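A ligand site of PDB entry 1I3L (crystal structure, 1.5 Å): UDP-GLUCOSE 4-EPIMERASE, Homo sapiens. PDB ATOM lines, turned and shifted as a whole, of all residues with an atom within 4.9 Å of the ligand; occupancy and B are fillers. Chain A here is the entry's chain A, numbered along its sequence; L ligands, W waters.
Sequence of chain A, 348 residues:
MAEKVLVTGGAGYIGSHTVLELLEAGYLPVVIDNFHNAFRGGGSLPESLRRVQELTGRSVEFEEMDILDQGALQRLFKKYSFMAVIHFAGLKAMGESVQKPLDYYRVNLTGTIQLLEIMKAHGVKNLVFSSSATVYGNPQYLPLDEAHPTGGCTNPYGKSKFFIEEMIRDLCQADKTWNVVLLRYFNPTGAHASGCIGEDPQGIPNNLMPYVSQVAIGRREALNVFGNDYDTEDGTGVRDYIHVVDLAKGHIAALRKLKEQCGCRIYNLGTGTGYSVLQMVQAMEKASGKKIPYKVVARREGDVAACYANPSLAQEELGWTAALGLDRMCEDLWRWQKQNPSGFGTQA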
ATOM      1  N   ALA A  93      28.130 -22.554  30.318  1.00  0.00           N
ATOM      2  CA  ALA A  93      26.898 -21.911  30.611  1.00  0.00           C
ATOM      3  C   ALA A  93      25.659 -22.718  30.425  1.00  0.00           C
ATOM      4  O   ALA A  93      25.605 -23.602  29.588  1.00  0.00           O
ATOM      5  CB  ALA A  93      26.807 -20.481  30.127  1.00  0.00           C
ATOM      6  N   GLY A  95      23.177 -21.313  29.605  1.00  0.00           N
ATOM      7  CA  GLY A  95      22.622 -20.252  28.778  1.00  0.00           C
ATOM      8  C   GLY A  95      22.641 -18.932  29.588  1.00  0.00           C
ATOM      9  O   GLY A  95      22.022 -17.934  29.224  1.00  0.00           O
ATOM     10  N   THR A 134      33.338 -22.878  20.431  1.00  0.00           N
ATOM     11  CA  THR A 134      32.620 -21.626  20.409  1.00  0.00           C
ATOM     12  C   THR A 134      33.491 -20.437  20.073  1.00  0.00           C
ATOM     13  O   THR A 134      32.989 -19.404  19.644  1.00  0.00           O
ATOM     14  CB  THR A 134      31.848 -21.307  21.706  1.00  0.00           C
ATOM     15  OG1 THR A 134      32.778 -21.239  22.758  1.00  0.00           O
ATOM     16  CG2 THR A 134      30.828 -22.412  21.953  1.00  0.00           C
ATOM     17  N   ASN A 155      28.629 -14.888  23.152  1.00  0.00           N
ATOM     18  CA  ASN A 155      28.410 -14.615  24.536  1.00  0.00           C
ATOM     19  C   ASN A 155      29.683 -14.480  25.357  1.00  0.00           C
ATOM     20  O   ASN A 155      30.808 -14.770  24.934  1.00  0.00           O
ATOM     21  CB  ASN A 155      27.536 -15.762  25.050  1.00  0.00           C
ATOM     22  CG  ASN A 155      28.188 -17.097  24.774  1.00  0.00           C
ATOM     23  OD1 ASN A 155      27.649 -17.872  23.989  1.00  0.00           O
ATOM     24  ND2 ASN A 155      29.339 -17.404  25.368  1.00  0.00           N
ATOM     25  N   ASN A 187      31.386 -31.176  20.909  1.00  0.00           N
ATOM     26  CA  ASN A 187      30.246 -31.466  21.832  1.00  0.00           C
ATOM     27  C   ASN A 187      30.443 -32.789  22.579  1.00  0.00           C
ATOM     28  O   ASN A 187      30.046 -33.857  22.107  1.00  0.00           O
ATOM     29  CB  ASN A 187      28.917 -31.484  21.057  1.00  0.00           C
ATOM     30  CG  ASN A 187      28.539 -30.073  20.659  1.00  0.00           C
ATOM     31  OD1 ASN A 187      29.311 -29.433  19.946  1.00  0.00           O
ATOM     32  ND2 ASN A 187      27.429 -29.550  21.166  1.00  0.00           N
ATOM     33  N   ASN A 206      20.641 -28.185  30.255  1.00  0.00           N
ATOM     34  CA  ASN A 206      20.644 -27.172  29.231  1.00  0.00           C
ATOM     35  C   ASN A 206      21.155 -27.719  27.903  1.00  0.00           C
ATOM     36  O   ASN A 206      20.880 -27.165  26.842  1.00  0.00           O
ATOM     37  CB  ASN A 206      21.286 -25.868  29.677  1.00  0.00           C
ATOM     38  CG  ASN A 206      20.668 -25.414  30.977  1.00  0.00           C
ATOM     39  OD1 ASN A 206      19.671 -24.669  30.989  1.00  0.00           O
ATOM     40  ND2 ASN A 206      21.240 -25.904  32.077  1.00  0.00           N
ATOM     41  N   ASN A 207      21.876 -28.835  27.983  1.00  0.00           N
ATOM     42  CA  ASN A 207      22.439 -29.501  26.826  1.00  0.00           C
ATOM     43  C   ASN A 207      21.572 -30.644  26.327  1.00  0.00           C
ATOM     44  O   ASN A 207      20.797 -31.227  27.069  1.00  0.00           O
ATOM     45  CB  ASN A 207      23.937 -29.874  26.906  1.00  0.00           C
ATOM     46  CG  ASN A 207      24.332 -30.624  28.164  1.00  0.00           C
ATOM     47  OD1 ASN A 207      23.756 -30.393  29.237  1.00  0.00           O
ATOM     48  ND2 ASN A 207      25.313 -31.496  28.028  1.00  0.00           N
ATOM     49  N   LEU A 208      21.744 -30.955  25.058  1.00  0.00           N
ATOM     50  CA  LEU A 208      20.949 -31.972  24.403  1.00  0.00           C
ATOM     51  C   LEU A 208      20.870 -33.368  24.982  1.00  0.00           C
ATOM     52  O   LEU A 208      19.800 -33.874  25.360  1.00  0.00           O
ATOM     53  CB  LEU A 208      21.361 -32.080  22.910  1.00  0.00           C
ATOM     54  CG  LEU A 208      20.500 -33.044  22.102  1.00  0.00           C
ATOM     55  CD1 LEU A 208      19.044 -32.577  22.043  1.00  0.00           C
ATOM     56  CD2 LEU A 208      21.047 -33.142  20.672  1.00  0.00           C
ATOM     57  N   TYR A 211      19.301 -34.318  28.314  1.00  0.00           N
ATOM     58  CA  TYR A 211      17.890 -34.133  28.228  1.00  0.00           C
ATOM     59  C   TYR A 211      17.295 -35.333  27.525  1.00  0.00           C
ATOM     60  O   TYR A 211      16.325 -35.945  27.962  1.00  0.00           O
ATOM     61  CB  TYR A 211      17.538 -32.824  27.542  1.00  0.00           C
ATOM     62  CG  TYR A 211      16.187 -32.357  27.994  1.00  0.00           C
ATOM     63  CD1 TYR A 211      15.032 -32.987  27.509  1.00  0.00           C
ATOM     64  CD2 TYR A 211      16.039 -31.294  28.889  1.00  0.00           C
ATOM     65  CE1 TYR A 211      13.755 -32.568  27.889  1.00  0.00           C
ATOM     66  CE2 TYR A 211      14.778 -30.851  29.281  1.00  0.00           C
ATOM     67  CZ  TYR A 211      13.648 -31.512  28.793  1.00  0.00           C
ATOM     68  OH  TYR A 211      12.363 -31.159  29.127  1.00  0.00           O
ATOM     69  N   LEU A 223      11.295 -34.372  24.542  1.00  0.00           N
ATOM     70  CA  LEU A 223      12.398 -33.467  24.263  1.00  0.00           C
ATOM     71  C   LEU A 223      11.853 -32.224  23.598  1.00  0.00           C
ATOM     72  O   LEU A 223      11.003 -32.326  22.723  1.00  0.00           O
ATOM     73  CB  LEU A 223      13.416 -34.141  23.298  1.00  0.00           C
ATOM     74  CG  LEU A 223      14.415 -33.162  22.654  1.00  0.00           C
ATOM     75  CD1 LEU A 223      15.454 -32.699  23.694  1.00  0.00           C
ATOM     76  CD2 LEU A 223      15.161 -33.840  21.523  1.00  0.00           C
ATOM     77  N   ASN A 224      12.341 -31.035  23.984  1.00  0.00           N
ATOM     78  CA  ASN A 224      11.937 -29.809  23.332  1.00  0.00           C
ATOM     79  C   ASN A 224      13.035 -29.555  22.308  1.00  0.00           C
ATOM     80  O   ASN A 224      14.182 -29.382  22.702  1.00  0.00           O
ATOM     81  CB  ASN A 224      11.823 -28.580  24.238  1.00  0.00           C
ATOM     82  CG  ASN A 224      10.518 -28.561  25.021  1.00  0.00           C
ATOM     83  OD1 ASN A 224      10.241 -27.623  25.772  1.00  0.00           O
ATOM     84  ND2 ASN A 224       9.707 -29.607  24.844  1.00  0.00           N
ATOM     85  N   VAL A 225      12.708 -29.581  21.027  1.00  0.00           N
ATOM     86  CA  VAL A 225      13.682 -29.369  19.965  1.00  0.00           C
ATOM     87  C   VAL A 225      13.735 -27.882  19.639  1.00  0.00           C
ATOM     88  O   VAL A 225      12.728 -27.291  19.247  1.00  0.00           O
ATOM     89  CB  VAL A 225      13.312 -30.203  18.738  1.00  0.00           C
ATOM     90  CG1 VAL A 225      14.123 -29.731  17.521  1.00  0.00           C
ATOM     91  CG2 VAL A 225      13.574 -31.690  19.000  1.00  0.00           C
ATOM     92  N   PHE A 226      14.902 -27.249  19.844  1.00  0.00           N
ATOM     93  CA  PHE A 226      15.027 -25.806  19.622  1.00  0.00           C
ATOM     94  C   PHE A 226      15.080 -25.346  18.175  1.00  0.00           C
ATOM     95  O   PHE A 226      16.133 -24.944  17.691  1.00  0.00           O
ATOM     96  CB  PHE A 226      16.259 -25.192  20.342  1.00  0.00           C
ATOM     97  CG  PHE A 226      16.290 -25.474  21.818  1.00  0.00           C
ATOM     98  CD1 PHE A 226      17.498 -25.593  22.502  1.00  0.00           C
ATOM     99  CD2 PHE A 226      15.093 -25.656  22.521  1.00  0.00           C
ATOM    100  CE1 PHE A 226      17.531 -25.874  23.870  1.00  0.00           C
ATOM    101  CE2 PHE A 226      15.106 -25.939  23.882  1.00  0.00           C
ATOM    102  CZ  PHE A 226      16.332 -26.054  24.551  1.00  0.00           C
ATOM    103  N   GLY A 237      19.540 -28.384  14.418  1.00  0.00           N
ATOM    104  CA  GLY A 237      20.967 -28.099  14.536  1.00  0.00           C
ATOM    105  C   GLY A 237      21.863 -29.318  14.379  1.00  0.00           C
ATOM    106  O   GLY A 237      21.524 -30.436  14.759  1.00  0.00           O
ATOM    107  N   VAL A 238      23.048 -29.083  13.800  1.00  0.00           N
ATOM    108  CA  VAL A 238      24.037 -30.117  13.568  1.00  0.00           C
ATOM    109  C   VAL A 238      25.279 -29.869  14.419  1.00  0.00           C
ATOM    110  O   VAL A 238      25.785 -28.742  14.450  1.00  0.00           O
ATOM    111  CB  VAL A 238      24.405 -30.235  12.071  1.00  0.00           C
ATOM    112  CG1 VAL A 238      25.587 -31.171  11.872  1.00  0.00           C
ATOM    113  CG2 VAL A 238      23.214 -30.756  11.274  1.00  0.00           C
ATOM    114  N   ARG A 239      25.761 -30.905  15.069  1.00  0.00           N
ATOM    115  CA  ARG A 239      26.954 -30.761  15.926  1.00  0.00           C
ATOM    116  C   ARG A 239      27.849 -31.964  15.851  1.00  0.00           C
ATOM    117  O   ARG A 239      27.412 -33.068  15.530  1.00  0.00           O
ATOM    118  CB  ARG A 239      26.562 -30.608  17.396  1.00  0.00           C
ATOM    119  CG  ARG A 239      25.613 -29.460  17.699  1.00  0.00           C
ATOM    120  CD  ARG A 239      26.335 -28.120  17.590  1.00  0.00           C
ATOM    121  NE  ARG A 239      25.481 -26.992  17.946  1.00  0.00           N
ATOM    122  CZ  ARG A 239      24.726 -26.269  17.123  1.00  0.00           C
ATOM    123  NH1 ARG A 239      24.658 -26.511  15.832  1.00  0.00           N
ATOM    124  NH2 ARG A 239      24.022 -25.270  17.631  1.00  0.00           N
ATOM    125  N   TYR A 241      29.424 -34.510  17.822  1.00  0.00           N
ATOM    126  CA  TYR A 241      29.411 -35.117  19.144  1.00  0.00           C
ATOM    127  C   TYR A 241      30.630 -35.987  19.294  1.00  0.00           C
ATOM    128  O   TYR A 241      30.936 -36.756  18.380  1.00  0.00           O
ATOM    129  CB  TYR A 241      28.097 -35.896  19.318  1.00  0.00           C
ATOM    130  CG  TYR A 241      26.944 -34.918  19.353  1.00  0.00           C
ATOM    131  CD1 TYR A 241      26.643 -34.184  20.509  1.00  0.00           C
ATOM    132  CD2 TYR A 241      26.132 -34.731  18.235  1.00  0.00           C
ATOM    133  CE1 TYR A 241      25.621 -33.256  20.542  1.00  0.00           C
ATOM    134  CE2 TYR A 241      25.087 -33.805  18.240  1.00  0.00           C
ATOM    135  CZ  TYR A 241      24.841 -33.054  19.395  1.00  0.00           C
ATOM    136  OH  TYR A 241      23.849 -32.127  19.426  1.00  0.00           O
ATOM    137  N   VAL A 277      19.896 -32.921  15.592  1.00  0.00           N
ATOM    138  CA  VAL A 277      19.136 -33.185  16.806  1.00  0.00           C
ATOM    139  C   VAL A 277      18.331 -34.482  16.633  1.00  0.00           C
ATOM    140  O   VAL A 277      18.409 -35.421  17.454  1.00  0.00           O
ATOM    141  CB  VAL A 277      18.245 -31.992  17.119  1.00  0.00           C
ATOM    142  CG1 VAL A 277      17.346 -32.314  18.318  1.00  0.00           C
ATOM    143  CG2 VAL A 277      19.121 -30.771  17.440  1.00  0.00           C
ATOM    144  N   ARG A 300      16.698 -21.322  19.988  1.00  0.00           N
ATOM    145  CA  ARG A 300      17.341 -20.872  21.206  1.00  0.00           C
ATOM    146  C   ARG A 300      18.292 -19.781  20.827  1.00  0.00           C
ATOM    147  O   ARG A 300      19.117 -19.989  19.941  1.00  0.00           O
ATOM    148  CB  ARG A 300      18.156 -21.989  21.848  1.00  0.00           C
ATOM    149  CG  ARG A 300      18.807 -21.569  23.168  1.00  0.00           C
ATOM    150  CD  ARG A 300      19.402 -22.758  23.919  1.00  0.00           C
ATOM    151  NE  ARG A 300      20.424 -23.489  23.154  1.00  0.00           N
ATOM    152  CZ  ARG A 300      21.022 -24.632  23.529  1.00  0.00           C
ATOM    153  NH1 ARG A 300      20.747 -25.235  24.679  1.00  0.00           N
ATOM    154  NH2 ARG A 300      21.910 -25.198  22.738  1.00  0.00           N
ATOM    155  N   ASP A 303      21.998 -19.906  18.994  1.00  0.00           N
ATOM    156  CA  ASP A 303      22.342 -21.180  18.401  1.00  0.00           C
ATOM    157  C   ASP A 303      22.798 -21.093  16.964  1.00  0.00           C
ATOM    158  O   ASP A 303      22.159 -20.383  16.170  1.00  0.00           O
ATOM    159  CB  ASP A 303      21.137 -22.124  18.419  1.00  0.00           C
ATOM    160  CG  ASP A 303      20.994 -22.867  19.691  1.00  0.00           C
ATOM    161  OD1 ASP A 303      21.726 -22.702  20.653  1.00  0.00           O
ATOM    162  OD2 ASP A 303      20.014 -23.736  19.612  1.00  0.00           O
ATOM    163  N   VAL A 304      23.851 -21.860  16.622  1.00  0.00           N
ATOM    164  CA  VAL A 304      24.321 -21.886  15.261  1.00  0.00           C
ATOM    165  C   VAL A 304      23.624 -23.020  14.507  1.00  0.00           C
ATOM    166  O   VAL A 304      23.157 -23.971  15.125  1.00  0.00           O
ATOM    167  CB  VAL A 304      25.851 -21.894  15.058  1.00  0.00           C
ATOM    168  CG1 VAL A 304      26.549 -20.846  15.903  1.00  0.00           C
ATOM    169  CG2 VAL A 304      26.472 -23.239  15.338  1.00  0.00           C
HETATM  170  N1  LIG L   1      19.053 -28.669  21.634  1.00  0.00           N
HETATM  171  C1  LIG L   1      17.667 -28.828  21.593  1.00  0.00           C
HETATM  172  N2  LIG L   1      17.088 -28.974  22.811  1.00  0.00           N
HETATM  173  C2  LIG L   1      17.717 -28.999  24.051  1.00  0.00           C
HETATM  174  C3  LIG L   1      19.124 -28.813  23.988  1.00  0.00           C
HETATM  175  C4  LIG L   1      19.742 -28.681  22.842  1.00  0.00           C
HETATM  176  O1  LIG L   1      16.967 -28.872  20.582  1.00  0.00           O
HETATM  177  O2  LIG L   1      17.047 -29.167  25.039  1.00  0.00           O
HETATM  178  C5  LIG L   1      19.828 -28.506  20.402  1.00  0.00           C
HETATM  179  C6  LIG L   1      20.553 -27.187  20.264  1.00  0.00           C
HETATM  180  O3  LIG L   1      19.684 -26.226  19.609  1.00  0.00           O
HETATM  181  C7  LIG L   1      21.722 -27.551  19.326  1.00  0.00           C
HETATM  182  C8  LIG L   1      22.017 -28.978  19.748  1.00  0.00           C
HETATM  183  O4  LIG L   1      20.796 -29.502  20.362  1.00  0.00           O
HETATM  184  O5  LIG L   1      21.375 -27.541  17.931  1.00  0.00           O
HETATM  185  C9  LIG L   1      23.157 -29.083  20.746  1.00  0.00           C
HETATM  186  O6  LIG L   1      22.863 -28.126  21.782  1.00  0.00           O
HETATM  187  P1  LIG L   1      23.714 -28.194  23.147  1.00  0.00           P
HETATM  188  O7  LIG L   1      23.863 -29.557  23.682  1.00  0.00           O
HETATM  189  O8  LIG L   1      23.149 -27.182  24.060  1.00  0.00           O
HETATM  190  O9  LIG L   1      25.215 -27.689  22.618  1.00  0.00           O
HETATM  191  P2  LIG L   1      25.691 -26.415  21.816  1.00  0.00           P
HETATM  192  O10 LIG L   1      24.708 -25.964  20.782  1.00  0.00           O
HETATM  193  O11 LIG L   1      26.942 -26.931  21.210  1.00  0.00           O
HETATM  194  O12 LIG L   1      26.043 -25.123  22.722  1.00  0.00           O
HETATM  195  C10 LIG L   1      25.008 -24.210  22.801  1.00  0.00           C
HETATM  196  C11 LIG L   1      25.549 -22.788  22.843  1.00  0.00           C
HETATM  197  C12 LIG L   1      26.384 -22.520  24.077  1.00  0.00           C
HETATM  198  C13 LIG L   1      25.719 -23.109  25.307  1.00  0.00           C
HETATM  199  C14 LIG L   1      25.450 -24.557  25.017  1.00  0.00           C
HETATM  200  C15 LIG L   1      24.926 -25.334  26.191  1.00  0.00           C
HETATM  201  O13 LIG L   1      26.310 -22.463  21.671  1.00  0.00           O
HETATM  202  O14 LIG L   1      26.432 -21.111  24.302  1.00  0.00           O
HETATM  203  O15 LIG L   1      24.464 -22.475  25.525  1.00  0.00           O
HETATM  204  O16 LIG L   1      24.401 -24.524  24.053  1.00  0.00           O
HETATM  205  O17 LIG L   1      23.573 -25.660  25.938  1.00  0.00           O
HETATM  206  O   HOH W   1      26.218 -30.940  23.414  1.00  0.00           O
HETATM  207  O   HOH W   2      22.907 -20.748  21.852  1.00  0.00           O
HETATM  208  O   HOH W   3      29.142 -26.317  23.056  1.00  0.00           O
HETATM  209  O   HOH W   4      17.941 -27.210  16.752  1.00  0.00           O
HETATM  210  O   HOH W   5      17.398 -27.816  27.571  1.00  0.00           O
HETATM  211  O   HOH W   6      20.739 -25.068  16.398  1.00  0.00           O
HETATM  212  O   HOH W   7      25.630 -22.616  18.685  1.00  0.00           O
HETATM  213  O   HOH W   8      14.431 -30.042  25.893  1.00  0.00           O
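The backbone carbonyl oxygen of Asn 206 is in hydrogen-bond range of an oxygen (O17) of the ligand, 3.2 Å away.
An oxygen (O7) of the ligand is in hydrogen-bond range of the backbone NH (N) of Leu 208, at 2.9 Å.
O of Asn 224 is in hydrogen-bond range of N2 of the ligand, at 2.9 Å.
An oxygen (O8) of the ligand lies within salt-bridge range of the guanidinium group of Arg 300 (2.7 Å).
NE of Arg 239 lies within salt-bridge range of O10 of the ligand (3.1 Å).
The side-chain amide oxygen of Asn 155 sits at hydrogen-bond distance from an oxygen (O14) of the ligand (3.5 Å).
O11 of the ligand sits at hydrogen-bond distance from ND2 of Asn 187, 2.7 Å away.
N of Phe 226 is in hydrogen-bond range of O1 of the ligand.
An oxygen (O3) of the ligand sits at hydrogen-bond distance from the side-chain carboxylate (OD2) of Asp 303, at 2.5 Å.
NH2 of Arg 239 sits at hydrogen-bond distance from O of Val 304, at 3.0 Å.
NH1 of Arg 300 sits at hydrogen-bond distance from O of Asn 206 (2.9 Å).
O of Gly 237 sits at hydrogen-bond distance from N of Val 277, 3.1 Å away.
The guanidinium group (NE) of Arg 300 lies within salt-bridge range of the side-chain carboxylate (OD1) of Asp 303.
Ala 93 touches the ligand.
Asn 207 touches the ligand.
Val 225 touches the ligand.
CA of Gly 237 touches O5 of the ligand (3.5 Å).
OH of Tyr 241 touches C9 of the ligand, at 3.4 Å.
Val 277 touches the ligand.
Hydrophobic or aromatic side chains within 4 Å of the ligand: Leu 208, Phe 226 and Val 277.
Of the 21 residues printed, 15 come within 4 Å of the ligand.
The nearest printed residue that does not touch the ligand is Leu 223 (4.1 Å).
Water W1 bridges an oxygen (O7) of the ligand and the side-chain amide nitrogen of Asn 187.
Water W8 lies within hydrogen-bond range of O2 of the ligand (2.9 Å) and N of Asn 224 (3.0 Å).
Water W6 lies within hydrogen-bond range of O of Val 304 and O5 of the ligand.
Water W7 lies within hydrogen-bond range of N of Val 304, O13 of the ligand and NH2 of Arg 239.
Water W4 lies within hydrogen-bond range of the backbone carbonyl oxygen (O) of Phe 226 (3.0 Å), the backbone NH (N) of Gly 237 (3.1 Å) and an oxygen (O3) of the ligand (3.5 Å).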
